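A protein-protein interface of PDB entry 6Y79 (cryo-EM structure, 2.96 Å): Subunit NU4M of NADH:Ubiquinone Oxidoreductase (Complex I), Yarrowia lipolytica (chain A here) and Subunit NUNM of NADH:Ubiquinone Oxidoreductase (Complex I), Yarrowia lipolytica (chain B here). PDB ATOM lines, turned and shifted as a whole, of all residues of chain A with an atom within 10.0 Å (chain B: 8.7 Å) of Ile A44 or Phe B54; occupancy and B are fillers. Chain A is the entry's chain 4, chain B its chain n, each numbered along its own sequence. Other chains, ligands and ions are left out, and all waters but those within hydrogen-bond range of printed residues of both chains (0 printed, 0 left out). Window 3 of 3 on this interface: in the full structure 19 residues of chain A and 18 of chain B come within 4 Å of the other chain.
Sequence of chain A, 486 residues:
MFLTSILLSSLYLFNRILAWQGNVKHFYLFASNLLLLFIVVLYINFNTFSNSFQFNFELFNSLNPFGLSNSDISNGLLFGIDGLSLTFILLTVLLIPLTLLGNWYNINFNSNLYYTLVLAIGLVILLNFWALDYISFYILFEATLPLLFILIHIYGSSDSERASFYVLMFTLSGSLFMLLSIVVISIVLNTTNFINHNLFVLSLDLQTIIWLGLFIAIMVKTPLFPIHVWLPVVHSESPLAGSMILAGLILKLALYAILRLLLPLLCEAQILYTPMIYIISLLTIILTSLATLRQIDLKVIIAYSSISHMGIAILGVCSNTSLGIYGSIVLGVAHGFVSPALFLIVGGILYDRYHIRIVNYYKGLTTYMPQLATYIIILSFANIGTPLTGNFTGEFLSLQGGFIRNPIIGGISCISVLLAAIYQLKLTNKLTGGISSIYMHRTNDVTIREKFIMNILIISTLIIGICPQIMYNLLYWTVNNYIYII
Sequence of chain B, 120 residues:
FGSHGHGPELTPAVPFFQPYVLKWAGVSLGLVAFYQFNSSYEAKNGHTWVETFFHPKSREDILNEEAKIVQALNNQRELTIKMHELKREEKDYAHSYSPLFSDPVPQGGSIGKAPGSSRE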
ATOM      1  N   LEU A  36     -33.776   9.116  19.425  1.00  0.00           N
ATOM      2  CA  LEU A  36     -32.550   8.342  19.240  1.00  0.00           C
ATOM      3  C   LEU A  36     -32.022   7.788  20.547  1.00  0.00           C
ATOM      4  O   LEU A  36     -31.817   6.577  20.664  1.00  0.00           O
ATOM      5  CB  LEU A  36     -31.457   9.187  18.627  1.00  0.00           C
ATOM      6  CG  LEU A  36     -31.066   9.326  17.192  1.00  0.00           C
ATOM      7  CD1 LEU A  36     -29.934  10.222  17.381  1.00  0.00           C
ATOM      8  CD2 LEU A  36     -30.575   8.022  16.635  1.00  0.00           C
ATOM      9  N   LEU A  37     -31.786   8.667  21.533  1.00  0.00           N
ATOM     10  CA  LEU A  37     -31.211   8.232  22.804  1.00  0.00           C
ATOM     11  C   LEU A  37     -32.123   7.239  23.507  1.00  0.00           C
ATOM     12  O   LEU A  37     -31.643   6.280  24.118  1.00  0.00           O
ATOM     13  CB  LEU A  37     -30.928   9.440  23.710  1.00  0.00           C
ATOM     14  CG  LEU A  37     -30.050   9.255  24.972  1.00  0.00           C
ATOM     15  CD1 LEU A  37     -29.237  10.507  25.218  1.00  0.00           C
ATOM     16  CD2 LEU A  37     -30.826   8.923  26.249  1.00  0.00           C
ATOM     17  N   PHE A  38     -33.438   7.424  23.383  1.00  0.00           N
ATOM     18  CA  PHE A  38     -34.391   6.503  23.993  1.00  0.00           C
ATOM     19  C   PHE A  38     -34.327   5.121  23.360  1.00  0.00           C
ATOM     20  O   PHE A  38     -34.338   4.111  24.071  1.00  0.00           O
ATOM     21  CB  PHE A  38     -35.807   7.059  23.881  1.00  0.00           C
ATOM     22  CG  PHE A  38     -36.848   6.180  24.502  1.00  0.00           C
ATOM     23  CD1 PHE A  38     -36.960   6.099  25.881  1.00  0.00           C
ATOM     24  CD2 PHE A  38     -37.682   5.406  23.718  1.00  0.00           C
ATOM     25  CE1 PHE A  38     -37.894   5.272  26.462  1.00  0.00           C
ATOM     26  CE2 PHE A  38     -38.616   4.576  24.296  1.00  0.00           C
ATOM     27  CZ  PHE A  38     -38.722   4.511  25.672  1.00  0.00           C
ATOM     28  N   ILE A  39     -34.241   5.053  22.028  1.00  0.00           N
ATOM     29  CA  ILE A  39     -34.152   3.750  21.372  1.00  0.00           C
ATOM     30  C   ILE A  39     -32.811   3.077  21.667  1.00  0.00           C
ATOM     31  O   ILE A  39     -32.745   1.847  21.812  1.00  0.00           O
ATOM     32  CB  ILE A  39     -34.426   3.903  19.861  1.00  0.00           C
ATOM     33  CG1 ILE A  39     -35.850   4.405  19.624  1.00  0.00           C
ATOM     34  CG2 ILE A  39     -34.274   2.596  19.125  1.00  0.00           C
ATOM     35  CD1 ILE A  39     -36.926   3.557  20.251  1.00  0.00           C
ATOM     36  N   VAL A  40     -31.742   3.851  21.852  1.00  0.00           N
ATOM     37  CA  VAL A  40     -30.485   3.179  22.177  1.00  0.00           C
ATOM     38  C   VAL A  40     -30.470   2.721  23.647  1.00  0.00           C
ATOM     39  O   VAL A  40     -29.892   1.668  23.957  1.00  0.00           O
ATOM     40  CB  VAL A  40     -29.267   4.057  21.824  1.00  0.00           C
ATOM     41  CG1 VAL A  40     -27.983   3.247  21.888  1.00  0.00           C
ATOM     42  CG2 VAL A  40     -29.389   4.582  20.449  1.00  0.00           C
ATOM     43  N   VAL A  41     -31.135   3.449  24.558  1.00  0.00           N
ATOM     44  CA  VAL A  41     -31.315   2.938  25.921  1.00  0.00           C
ATOM     45  C   VAL A  41     -32.154   1.664  25.911  1.00  0.00           C
ATOM     46  O   VAL A  41     -31.859   0.713  26.643  1.00  0.00           O
ATOM     47  CB  VAL A  41     -31.913   4.021  26.842  1.00  0.00           C
ATOM     48  CG1 VAL A  41     -32.322   3.446  28.199  1.00  0.00           C
ATOM     49  CG2 VAL A  41     -30.894   5.142  27.078  1.00  0.00           C
ATOM     50  N   LEU A  42     -33.156   1.588  25.033  1.00  0.00           N
ATOM     51  CA  LEU A  42     -33.896   0.338  24.869  1.00  0.00           C
ATOM     52  C   LEU A  42     -33.027  -0.781  24.326  1.00  0.00           C
ATOM     53  O   LEU A  42     -33.242  -1.948  24.658  1.00  0.00           O
ATOM     54  CB  LEU A  42     -35.078   0.527  23.928  1.00  0.00           C
ATOM     55  CG  LEU A  42     -36.247   1.369  24.392  1.00  0.00           C
ATOM     56  CD1 LEU A  42     -37.281   1.285  23.327  1.00  0.00           C
ATOM     57  CD2 LEU A  42     -36.794   0.886  25.712  1.00  0.00           C
ATOM     58  N   TYR A  43     -32.063  -0.455  23.479  1.00  0.00           N
ATOM     59  CA  TYR A  43     -31.183  -1.485  22.943  1.00  0.00           C
ATOM     60  C   TYR A  43     -30.193  -1.973  23.999  1.00  0.00           C
ATOM     61  O   TYR A  43     -29.750  -3.126  23.955  1.00  0.00           O
ATOM     62  CB  TYR A  43     -30.482  -0.948  21.698  1.00  0.00           C
ATOM     63  CG  TYR A  43     -29.514  -1.916  21.068  1.00  0.00           C
ATOM     64  CD1 TYR A  43     -29.875  -3.228  20.842  1.00  0.00           C
ATOM     65  CD2 TYR A  43     -28.257  -1.516  20.696  1.00  0.00           C
ATOM     66  CE1 TYR A  43     -29.010  -4.122  20.285  1.00  0.00           C
ATOM     67  CE2 TYR A  43     -27.383  -2.381  20.118  1.00  0.00           C
ATOM     68  CZ  TYR A  43     -27.760  -3.689  19.910  1.00  0.00           C
ATOM     69  OH  TYR A  43     -26.895  -4.580  19.339  1.00  0.00           O
ATOM     70  N   ILE A  44     -29.851  -1.119  24.966  1.00  0.00           N
ATOM     71  CA  ILE A  44     -29.005  -1.547  26.084  1.00  0.00           C
ATOM     72  C   ILE A  44     -29.726  -2.584  26.939  1.00  0.00           C
ATOM     73  O   ILE A  44     -29.156  -3.617  27.314  1.00  0.00           O
ATOM     74  CB  ILE A  44     -28.572  -0.333  26.924  1.00  0.00           C
ATOM     75  CG1 ILE A  44     -27.682   0.593  26.108  1.00  0.00           C
ATOM     76  CG2 ILE A  44     -27.830  -0.765  28.159  1.00  0.00           C
ATOM     77  CD1 ILE A  44     -27.268   1.833  26.834  1.00  0.00           C
ATOM     78  N   ASN A  45     -31.001  -2.342  27.230  1.00  0.00           N
ATOM     79  CA  ASN A  45     -31.809  -3.228  28.059  1.00  0.00           C
ATOM     80  C   ASN A  45     -32.419  -4.392  27.290  1.00  0.00           C
ATOM     81  O   ASN A  45     -33.246  -5.113  27.849  1.00  0.00           O
ATOM     82  CB  ASN A  45     -32.920  -2.430  28.734  1.00  0.00           C
ATOM     83  CG  ASN A  45     -32.390  -1.447  29.737  1.00  0.00           C
ATOM     84  OD1 ASN A  45     -31.466  -1.748  30.489  1.00  0.00           O
ATOM     85  ND2 ASN A  45     -32.971  -0.258  29.757  1.00  0.00           N
ATOM     86  N   PHE A  46     -32.035  -4.594  26.039  1.00  0.00           N
ATOM     87  CA  PHE A  46     -32.609  -5.645  25.213  1.00  0.00           C
ATOM     88  C   PHE A  46     -31.918  -6.974  25.492  1.00  0.00           C
ATOM     89  O   PHE A  46     -30.688  -7.042  25.552  1.00  0.00           O
ATOM     90  CB  PHE A  46     -32.474  -5.259  23.740  1.00  0.00           C
ATOM     91  CG  PHE A  46     -33.074  -6.242  22.788  1.00  0.00           C
ATOM     92  CD1 PHE A  46     -34.425  -6.228  22.524  1.00  0.00           C
ATOM     93  CD2 PHE A  46     -32.279  -7.162  22.130  1.00  0.00           C
ATOM     94  CE1 PHE A  46     -34.973  -7.119  21.644  1.00  0.00           C
ATOM     95  CE2 PHE A  46     -32.828  -8.068  21.254  1.00  0.00           C
ATOM     96  CZ  PHE A  46     -34.177  -8.046  21.012  1.00  0.00           C
ATOM     97  N   ASN A  47     -32.705  -8.029  25.661  1.00  0.00           N
ATOM     98  CA  ASN A  47     -32.171  -9.367  25.879  1.00  0.00           C
ATOM     99  C   ASN A  47     -32.047 -10.078  24.540  1.00  0.00           C
ATOM    100  O   ASN A  47     -33.055 -10.406  23.912  1.00  0.00           O
ATOM    101  CB  ASN A  47     -33.066 -10.166  26.823  1.00  0.00           C
ATOM    102  CG  ASN A  47     -32.408 -11.441  27.318  1.00  0.00           C
ATOM    103  OD1 ASN A  47     -31.243 -11.705  27.046  1.00  0.00           O
ATOM    104  ND2 ASN A  47     -33.162 -12.244  28.044  1.00  0.00           N
ATOM    105  N   THR A  48     -30.812 -10.329  24.116  1.00  0.00           N
ATOM    106  CA  THR A  48     -30.584 -11.015  22.855  1.00  0.00           C
ATOM    107  C   THR A  48     -30.722 -12.522  22.983  1.00  0.00           C
ATOM    108  O   THR A  48     -30.882 -13.205  21.967  1.00  0.00           O
ATOM    109  CB  THR A  48     -29.199 -10.669  22.320  1.00  0.00           C
ATOM    110  OG1 THR A  48     -28.205 -11.207  23.197  1.00  0.00           O
ATOM    111  CG2 THR A  48     -29.029  -9.167  22.245  1.00  0.00           C
ATOM    112  N   GLN A  54     -39.860  -8.368  23.721  1.00  0.00           N
ATOM    113  CA  GLN A  54     -39.379  -7.919  25.023  1.00  0.00           C
ATOM    114  C   GLN A  54     -40.159  -6.745  25.599  1.00  0.00           C
ATOM    115  O   GLN A  54     -40.530  -6.775  26.778  1.00  0.00           O
ATOM    116  CB  GLN A  54     -37.893  -7.556  24.947  1.00  0.00           C
ATOM    117  CG  GLN A  54     -36.949  -8.736  25.003  1.00  0.00           C
ATOM    118  CD  GLN A  54     -36.795  -9.398  23.664  1.00  0.00           C
ATOM    119  OE1 GLN A  54     -37.320  -8.920  22.665  1.00  0.00           O
ATOM    120  NE2 GLN A  54     -36.076 -10.506  23.628  1.00  0.00           N
ATOM    121  N   PHE A  55     -40.393  -5.694  24.822  1.00  0.00           N
ATOM    122  CA  PHE A  55     -40.972  -4.467  25.368  1.00  0.00           C
ATOM    123  C   PHE A  55     -42.384  -4.323  24.820  1.00  0.00           C
ATOM    124  O   PHE A  55     -42.631  -3.580  23.876  1.00  0.00           O
ATOM    125  CB  PHE A  55     -40.110  -3.265  25.026  1.00  0.00           C
ATOM    126  CG  PHE A  55     -38.757  -3.289  25.669  1.00  0.00           C
ATOM    127  CD1 PHE A  55     -38.566  -3.906  26.889  1.00  0.00           C
ATOM    128  CD2 PHE A  55     -37.673  -2.716  25.046  1.00  0.00           C
ATOM    129  CE1 PHE A  55     -37.320  -3.938  27.477  1.00  0.00           C
ATOM    130  CE2 PHE A  55     -36.431  -2.747  25.633  1.00  0.00           C
ATOM    131  CZ  PHE A  55     -36.257  -3.355  26.846  1.00  0.00           C
ATOM    132  N   ILE A  81     -41.186  -5.710  20.276  1.00  0.00           N
ATOM    133  CA  ILE A  81     -40.053  -5.849  19.369  1.00  0.00           C
ATOM    134  C   ILE A  81     -39.321  -7.166  19.583  1.00  0.00           C
ATOM    135  O   ILE A  81     -39.268  -7.713  20.681  1.00  0.00           O
ATOM    136  CB  ILE A  81     -39.053  -4.687  19.506  1.00  0.00           C
ATOM    137  CG1 ILE A  81     -38.640  -4.493  20.954  1.00  0.00           C
ATOM    138  CG2 ILE A  81     -39.634  -3.427  18.986  1.00  0.00           C
ATOM    139  CD1 ILE A  81     -37.369  -3.725  21.099  1.00  0.00           C
ATOM    140  N   LEU A  86     -36.046  -4.385  15.767  1.00  0.00           N
ATOM    141  CA  LEU A  86     -35.182  -3.364  16.342  1.00  0.00           C
ATOM    142  C   LEU A  86     -34.064  -2.961  15.391  1.00  0.00           C
ATOM    143  O   LEU A  86     -33.579  -1.827  15.469  1.00  0.00           O
ATOM    144  CB  LEU A  86     -34.625  -3.868  17.669  1.00  0.00           C
ATOM    145  CG  LEU A  86     -33.712  -2.994  18.525  1.00  0.00           C
ATOM    146  CD1 LEU A  86     -34.448  -1.783  19.046  1.00  0.00           C
ATOM    147  CD2 LEU A  86     -33.218  -3.825  19.665  1.00  0.00           C
ATOM    148  N   LEU A  90     -33.610   0.980  14.618  1.00  0.00           N
ATOM    149  CA  LEU A  90     -32.361   1.737  14.705  1.00  0.00           C
ATOM    150  C   LEU A  90     -32.051   2.445  13.390  1.00  0.00           C
ATOM    151  O   LEU A  90     -31.661   3.626  13.387  1.00  0.00           O
ATOM    152  CB  LEU A  90     -31.207   0.818  15.103  1.00  0.00           C
ATOM    153  CG  LEU A  90     -31.177   0.151  16.479  1.00  0.00           C
ATOM    154  CD1 LEU A  90     -30.081  -0.894  16.542  1.00  0.00           C
ATOM    155  CD2 LEU A  90     -31.003   1.167  17.577  1.00  0.00           C
ATOM    156  N   ASN A 473     -26.056 -10.027  16.588  1.00  0.00           N
ATOM    157  CA  ASN A 473     -26.606 -10.304  17.910  1.00  0.00           C
ATOM    158  C   ASN A 473     -28.106 -10.062  17.992  1.00  0.00           C
ATOM    159  O   ASN A 473     -28.764 -10.593  18.890  1.00  0.00           O
ATOM    160  CB  ASN A 473     -25.901  -9.448  18.960  1.00  0.00           C
ATOM    161  CG  ASN A 473     -25.855  -7.981  18.586  1.00  0.00           C
ATOM    162  OD1 ASN A 473     -26.423  -7.558  17.591  1.00  0.00           O
ATOM    163  ND2 ASN A 473     -25.171  -7.201  19.388  1.00  0.00           N
ATOM    164  N   LEU A 474     -28.648  -9.254  17.095  1.00  0.00           N
ATOM    165  CA  LEU A 474     -30.082  -9.072  17.002  1.00  0.00           C
ATOM    166  C   LEU A 474     -30.738 -10.112  16.124  1.00  0.00           C
ATOM    167  O   LEU A 474     -31.913 -10.428  16.319  1.00  0.00           O
ATOM    168  CB  LEU A 474     -30.391  -7.686  16.454  1.00  0.00           C
ATOM    169  CG  LEU A 474     -29.946  -6.575  17.388  1.00  0.00           C
ATOM    170  CD1 LEU A 474     -30.072  -5.233  16.715  1.00  0.00           C
ATOM    171  CD2 LEU A 474     -30.814  -6.647  18.603  1.00  0.00           C
ATOM    172  N   THR B  48     -16.567  -7.433  31.093  1.00  0.00           N
ATOM    173  CA  THR B  48     -16.414  -6.126  30.461  1.00  0.00           C
ATOM    174  C   THR B  48     -16.955  -5.022  31.388  1.00  0.00           C
ATOM    175  O   THR B  48     -17.793  -5.267  32.258  1.00  0.00           O
ATOM    176  CB  THR B  48     -17.136  -6.167  29.102  1.00  0.00           C
ATOM    177  OG1 THR B  48     -16.648  -7.292  28.360  1.00  0.00           O
ATOM    178  CG2 THR B  48     -16.931  -4.920  28.236  1.00  0.00           C
ATOM    179  N   TRP B  49     -16.445  -3.795  31.217  1.00  0.00           N
ATOM    180  CA  TRP B  49     -16.974  -2.656  31.960  1.00  0.00           C
ATOM    181  C   TRP B  49     -18.328  -2.213  31.406  1.00  0.00           C
ATOM    182  O   TRP B  49     -19.134  -1.613  32.118  1.00  0.00           O
ATOM    183  CB  TRP B  49     -15.986  -1.488  31.935  1.00  0.00           C
ATOM    184  CG  TRP B  49     -16.480  -0.362  32.782  1.00  0.00           C
ATOM    185  CD1 TRP B  49     -16.586  -0.354  34.137  1.00  0.00           C
ATOM    186  CD2 TRP B  49     -17.012   0.888  32.331  1.00  0.00           C
ATOM    187  NE1 TRP B  49     -17.122   0.833  34.564  1.00  0.00           N
ATOM    188  CE2 TRP B  49     -17.392   1.615  33.473  1.00  0.00           C
ATOM    189  CE3 TRP B  49     -17.190   1.467  31.074  1.00  0.00           C
ATOM    190  CZ2 TRP B  49     -17.938   2.889  33.398  1.00  0.00           C
ATOM    191  CZ3 TRP B  49     -17.732   2.735  30.999  1.00  0.00           C
ATOM    192  CH2 TRP B  49     -18.100   3.434  32.155  1.00  0.00           C
ATOM    193  N   VAL B  50     -18.604  -2.476  30.130  1.00  0.00           N
ATOM    194  CA  VAL B  50     -19.875  -2.020  29.575  1.00  0.00           C
ATOM    195  C   VAL B  50     -20.994  -3.005  29.894  1.00  0.00           C
ATOM    196  O   VAL B  50     -22.136  -2.586  30.094  1.00  0.00           O
ATOM    197  CB  VAL B  50     -19.692  -1.737  28.071  1.00  0.00           C
ATOM    198  CG1 VAL B  50     -21.008  -1.488  27.346  1.00  0.00           C
ATOM    199  CG2 VAL B  50     -18.840  -0.521  27.916  1.00  0.00           C
ATOM    200  N   GLU B  51     -20.694  -4.298  30.069  1.00  0.00           N
ATOM    201  CA  GLU B  51     -21.751  -5.233  30.451  1.00  0.00           C
ATOM    202  C   GLU B  51     -22.149  -5.094  31.924  1.00  0.00           C
ATOM    203  O   GLU B  51     -23.080  -5.773  32.371  1.00  0.00           O
ATOM    204  CB  GLU B  51     -21.342  -6.667  30.117  1.00  0.00           C
ATOM    205  CG  GLU B  51     -20.281  -7.279  31.004  1.00  0.00           C
ATOM    206  CD  GLU B  51     -19.831  -8.647  30.514  1.00  0.00           C
ATOM    207  OE1 GLU B  51     -19.219  -8.721  29.432  1.00  0.00           O
ATOM    208  OE2 GLU B  51     -20.098  -9.651  31.203  1.00  0.00           O
ATOM    209  N   THR B  52     -21.457  -4.238  32.696  1.00  0.00           N
ATOM    210  CA  THR B  52     -22.023  -3.730  33.945  1.00  0.00           C
ATOM    211  C   THR B  52     -23.363  -3.049  33.710  1.00  0.00           C
ATOM    212  O   THR B  52     -24.281  -3.185  34.524  1.00  0.00           O
ATOM    213  CB  THR B  52     -21.088  -2.715  34.604  1.00  0.00           C
ATOM    214  OG1 THR B  52     -20.928  -1.582  33.732  1.00  0.00           O
ATOM    215  CG2 THR B  52     -19.733  -3.315  34.915  1.00  0.00           C
ATOM    216  N   PHE B  53     -23.489  -2.297  32.616  1.00  0.00           N
ATOM    217  CA  PHE B  53     -24.684  -1.516  32.326  1.00  0.00           C
ATOM    218  C   PHE B  53     -25.735  -2.302  31.562  1.00  0.00           C
ATOM    219  O   PHE B  53     -26.841  -1.794  31.366  1.00  0.00           O
ATOM    220  CB  PHE B  53     -24.320  -0.263  31.522  1.00  0.00           C
ATOM    221  CG  PHE B  53     -23.464   0.722  32.270  1.00  0.00           C
ATOM    222  CD1 PHE B  53     -23.421   0.735  33.658  1.00  0.00           C
ATOM    223  CD2 PHE B  53     -22.695   1.637  31.575  1.00  0.00           C
ATOM    224  CE1 PHE B  53     -22.627   1.645  34.330  1.00  0.00           C
ATOM    225  CE2 PHE B  53     -21.903   2.547  32.238  1.00  0.00           C
ATOM    226  CZ  PHE B  53     -21.868   2.552  33.619  1.00  0.00           C
ATOM    227  N   PHE B  54     -25.415  -3.508  31.111  1.00  0.00           N
ATOM    228  CA  PHE B  54     -26.376  -4.338  30.395  1.00  0.00           C
ATOM    229  C   PHE B  54     -27.264  -4.990  31.435  1.00  0.00           C
ATOM    230  O   PHE B  54     -26.851  -5.931  32.117  1.00  0.00           O
ATOM    231  CB  PHE B  54     -25.684  -5.400  29.546  1.00  0.00           C
ATOM    232  CG  PHE B  54     -24.934  -4.865  28.362  1.00  0.00           C
ATOM    233  CD1 PHE B  54     -25.073  -3.551  27.944  1.00  0.00           C
ATOM    234  CD2 PHE B  54     -24.093  -5.701  27.653  1.00  0.00           C
ATOM    235  CE1 PHE B  54     -24.374  -3.083  26.859  1.00  0.00           C
ATOM    236  CE2 PHE B  54     -23.395  -5.239  26.568  1.00  0.00           C
ATOM    237  CZ  PHE B  54     -23.536  -3.928  26.171  1.00  0.00           C
ATOM    238  N   HIS B  55     -28.494  -4.499  31.564  1.00  0.00           N
ATOM    239  CA  HIS B  55     -29.475  -5.082  32.474  1.00  0.00           C
ATOM    240  C   HIS B  55     -30.744  -5.439  31.711  1.00  0.00           C
ATOM    241  O   HIS B  55     -31.740  -4.703  31.774  1.00  0.00           O
ATOM    242  CB  HIS B  55     -29.790  -4.133  33.627  1.00  0.00           C
ATOM    243  CG  HIS B  55     -28.631  -3.893  34.539  1.00  0.00           C
ATOM    244  ND1 HIS B  55     -28.149  -4.858  35.395  1.00  0.00           N
ATOM    245  CD2 HIS B  55     -27.853  -2.801  34.724  1.00  0.00           C
ATOM    246  CE1 HIS B  55     -27.125  -4.371  36.071  1.00  0.00           C
ATOM    247  NE2 HIS B  55     -26.923  -3.125  35.681  1.00  0.00           N
ATOM    248  N   PRO B  56     -30.757  -6.557  30.992  1.00  0.00           N
ATOM    249  CA  PRO B  56     -32.021  -7.070  30.472  1.00  0.00           C
ATOM    250  C   PRO B  56     -32.683  -8.001  31.477  1.00  0.00           C
ATOM    251  O   PRO B  56     -32.058  -8.501  32.414  1.00  0.00           O
ATOM    252  CB  PRO B  56     -31.580  -7.832  29.221  1.00  0.00           C
ATOM    253  CG  PRO B  56     -30.269  -8.379  29.596  1.00  0.00           C
ATOM    254  CD  PRO B  56     -29.626  -7.382  30.523  1.00  0.00           C
ATOM    255  N   LYS B  57     -33.977  -8.212  31.275  1.00  0.00           N
ATOM    256  CA  LYS B  57     -34.695  -9.179  32.086  1.00  0.00           C
ATOM    257  C   LYS B  57     -34.228 -10.587  31.746  1.00  0.00           C
ATOM    258  O   LYS B  57     -33.734 -10.848  30.646  1.00  0.00           O
ATOM    259  CB  LYS B  57     -36.197  -9.056  31.854  1.00  0.00           C
ATOM    260  CG  LYS B  57     -36.773  -7.712  32.212  1.00  0.00           C
ATOM    261  CD  LYS B  57     -38.265  -7.699  31.975  1.00  0.00           C
ATOM    262  CE  LYS B  57     -38.873  -6.377  32.380  1.00  0.00           C
ATOM    263  NZ  LYS B  57     -40.332  -6.337  32.102  1.00  0.00           N
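The backbone carbonyl oxygen (O) of Lys B57 sits at hydrogen-bond distance from the side-chain amide nitrogen (ND2) of Asn A47.
The backbone carbonyl oxygen (O) of His B55 sits close to the side-chain amide oxygen (OD1) of Asn A45 (3.2 Å).
The backbone carbonyl oxygen (O) of Asn A47 lies within hydrogen-bond range of the side-chain amide nitrogen (NE2) of Gln A54 (3.0 Å).
O of Thr B52 sits at hydrogen-bond distance from NE2 of His B55.
O of Val A41 lies within hydrogen-bond range of ND2 of Asn A45, at 3.4 Å.
Among the printed residues, pairs that only touch across the chains: Asn A45 with Pro B56, Ile A44 with Phe B53, Asn A47 with Pro B56, Phe A46 with Pro B56 and Ile A44 with Phe B54.
Of chain B, only Phe B53 and Phe B54 come within 4 Å of Ile A44.
Of the printed residues of chain B, Asn A47 touches Pro B56 and Lys B57.
Printed residues of chain A within 4 Å of Phe B53: Ile A44.
Of chain A, only Ile A44 comes within 4 Å of Phe B54.
Printed residues of chain A within 4 Å of His B55: Asn A45 (3.2 Å).
Printed residues of chain A within 4 Å of Pro B56: Asn A45, Phe A46 and Asn A47.
The nearest printed residue of chain A that does not touch Phe B53 is Asn A45 (4.7 Å).
Hydrophobic or aromatic side chains of chain A that line the printed part of chain B: Ile A44.
Along chain B the printed residues that touch a printed residue of chain A span positions 53 to 57.
Among the printed residues, no Asp or Glu carboxylate lies within 4 Å of a Lys or Arg side-chain nitrogen of the other chain.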
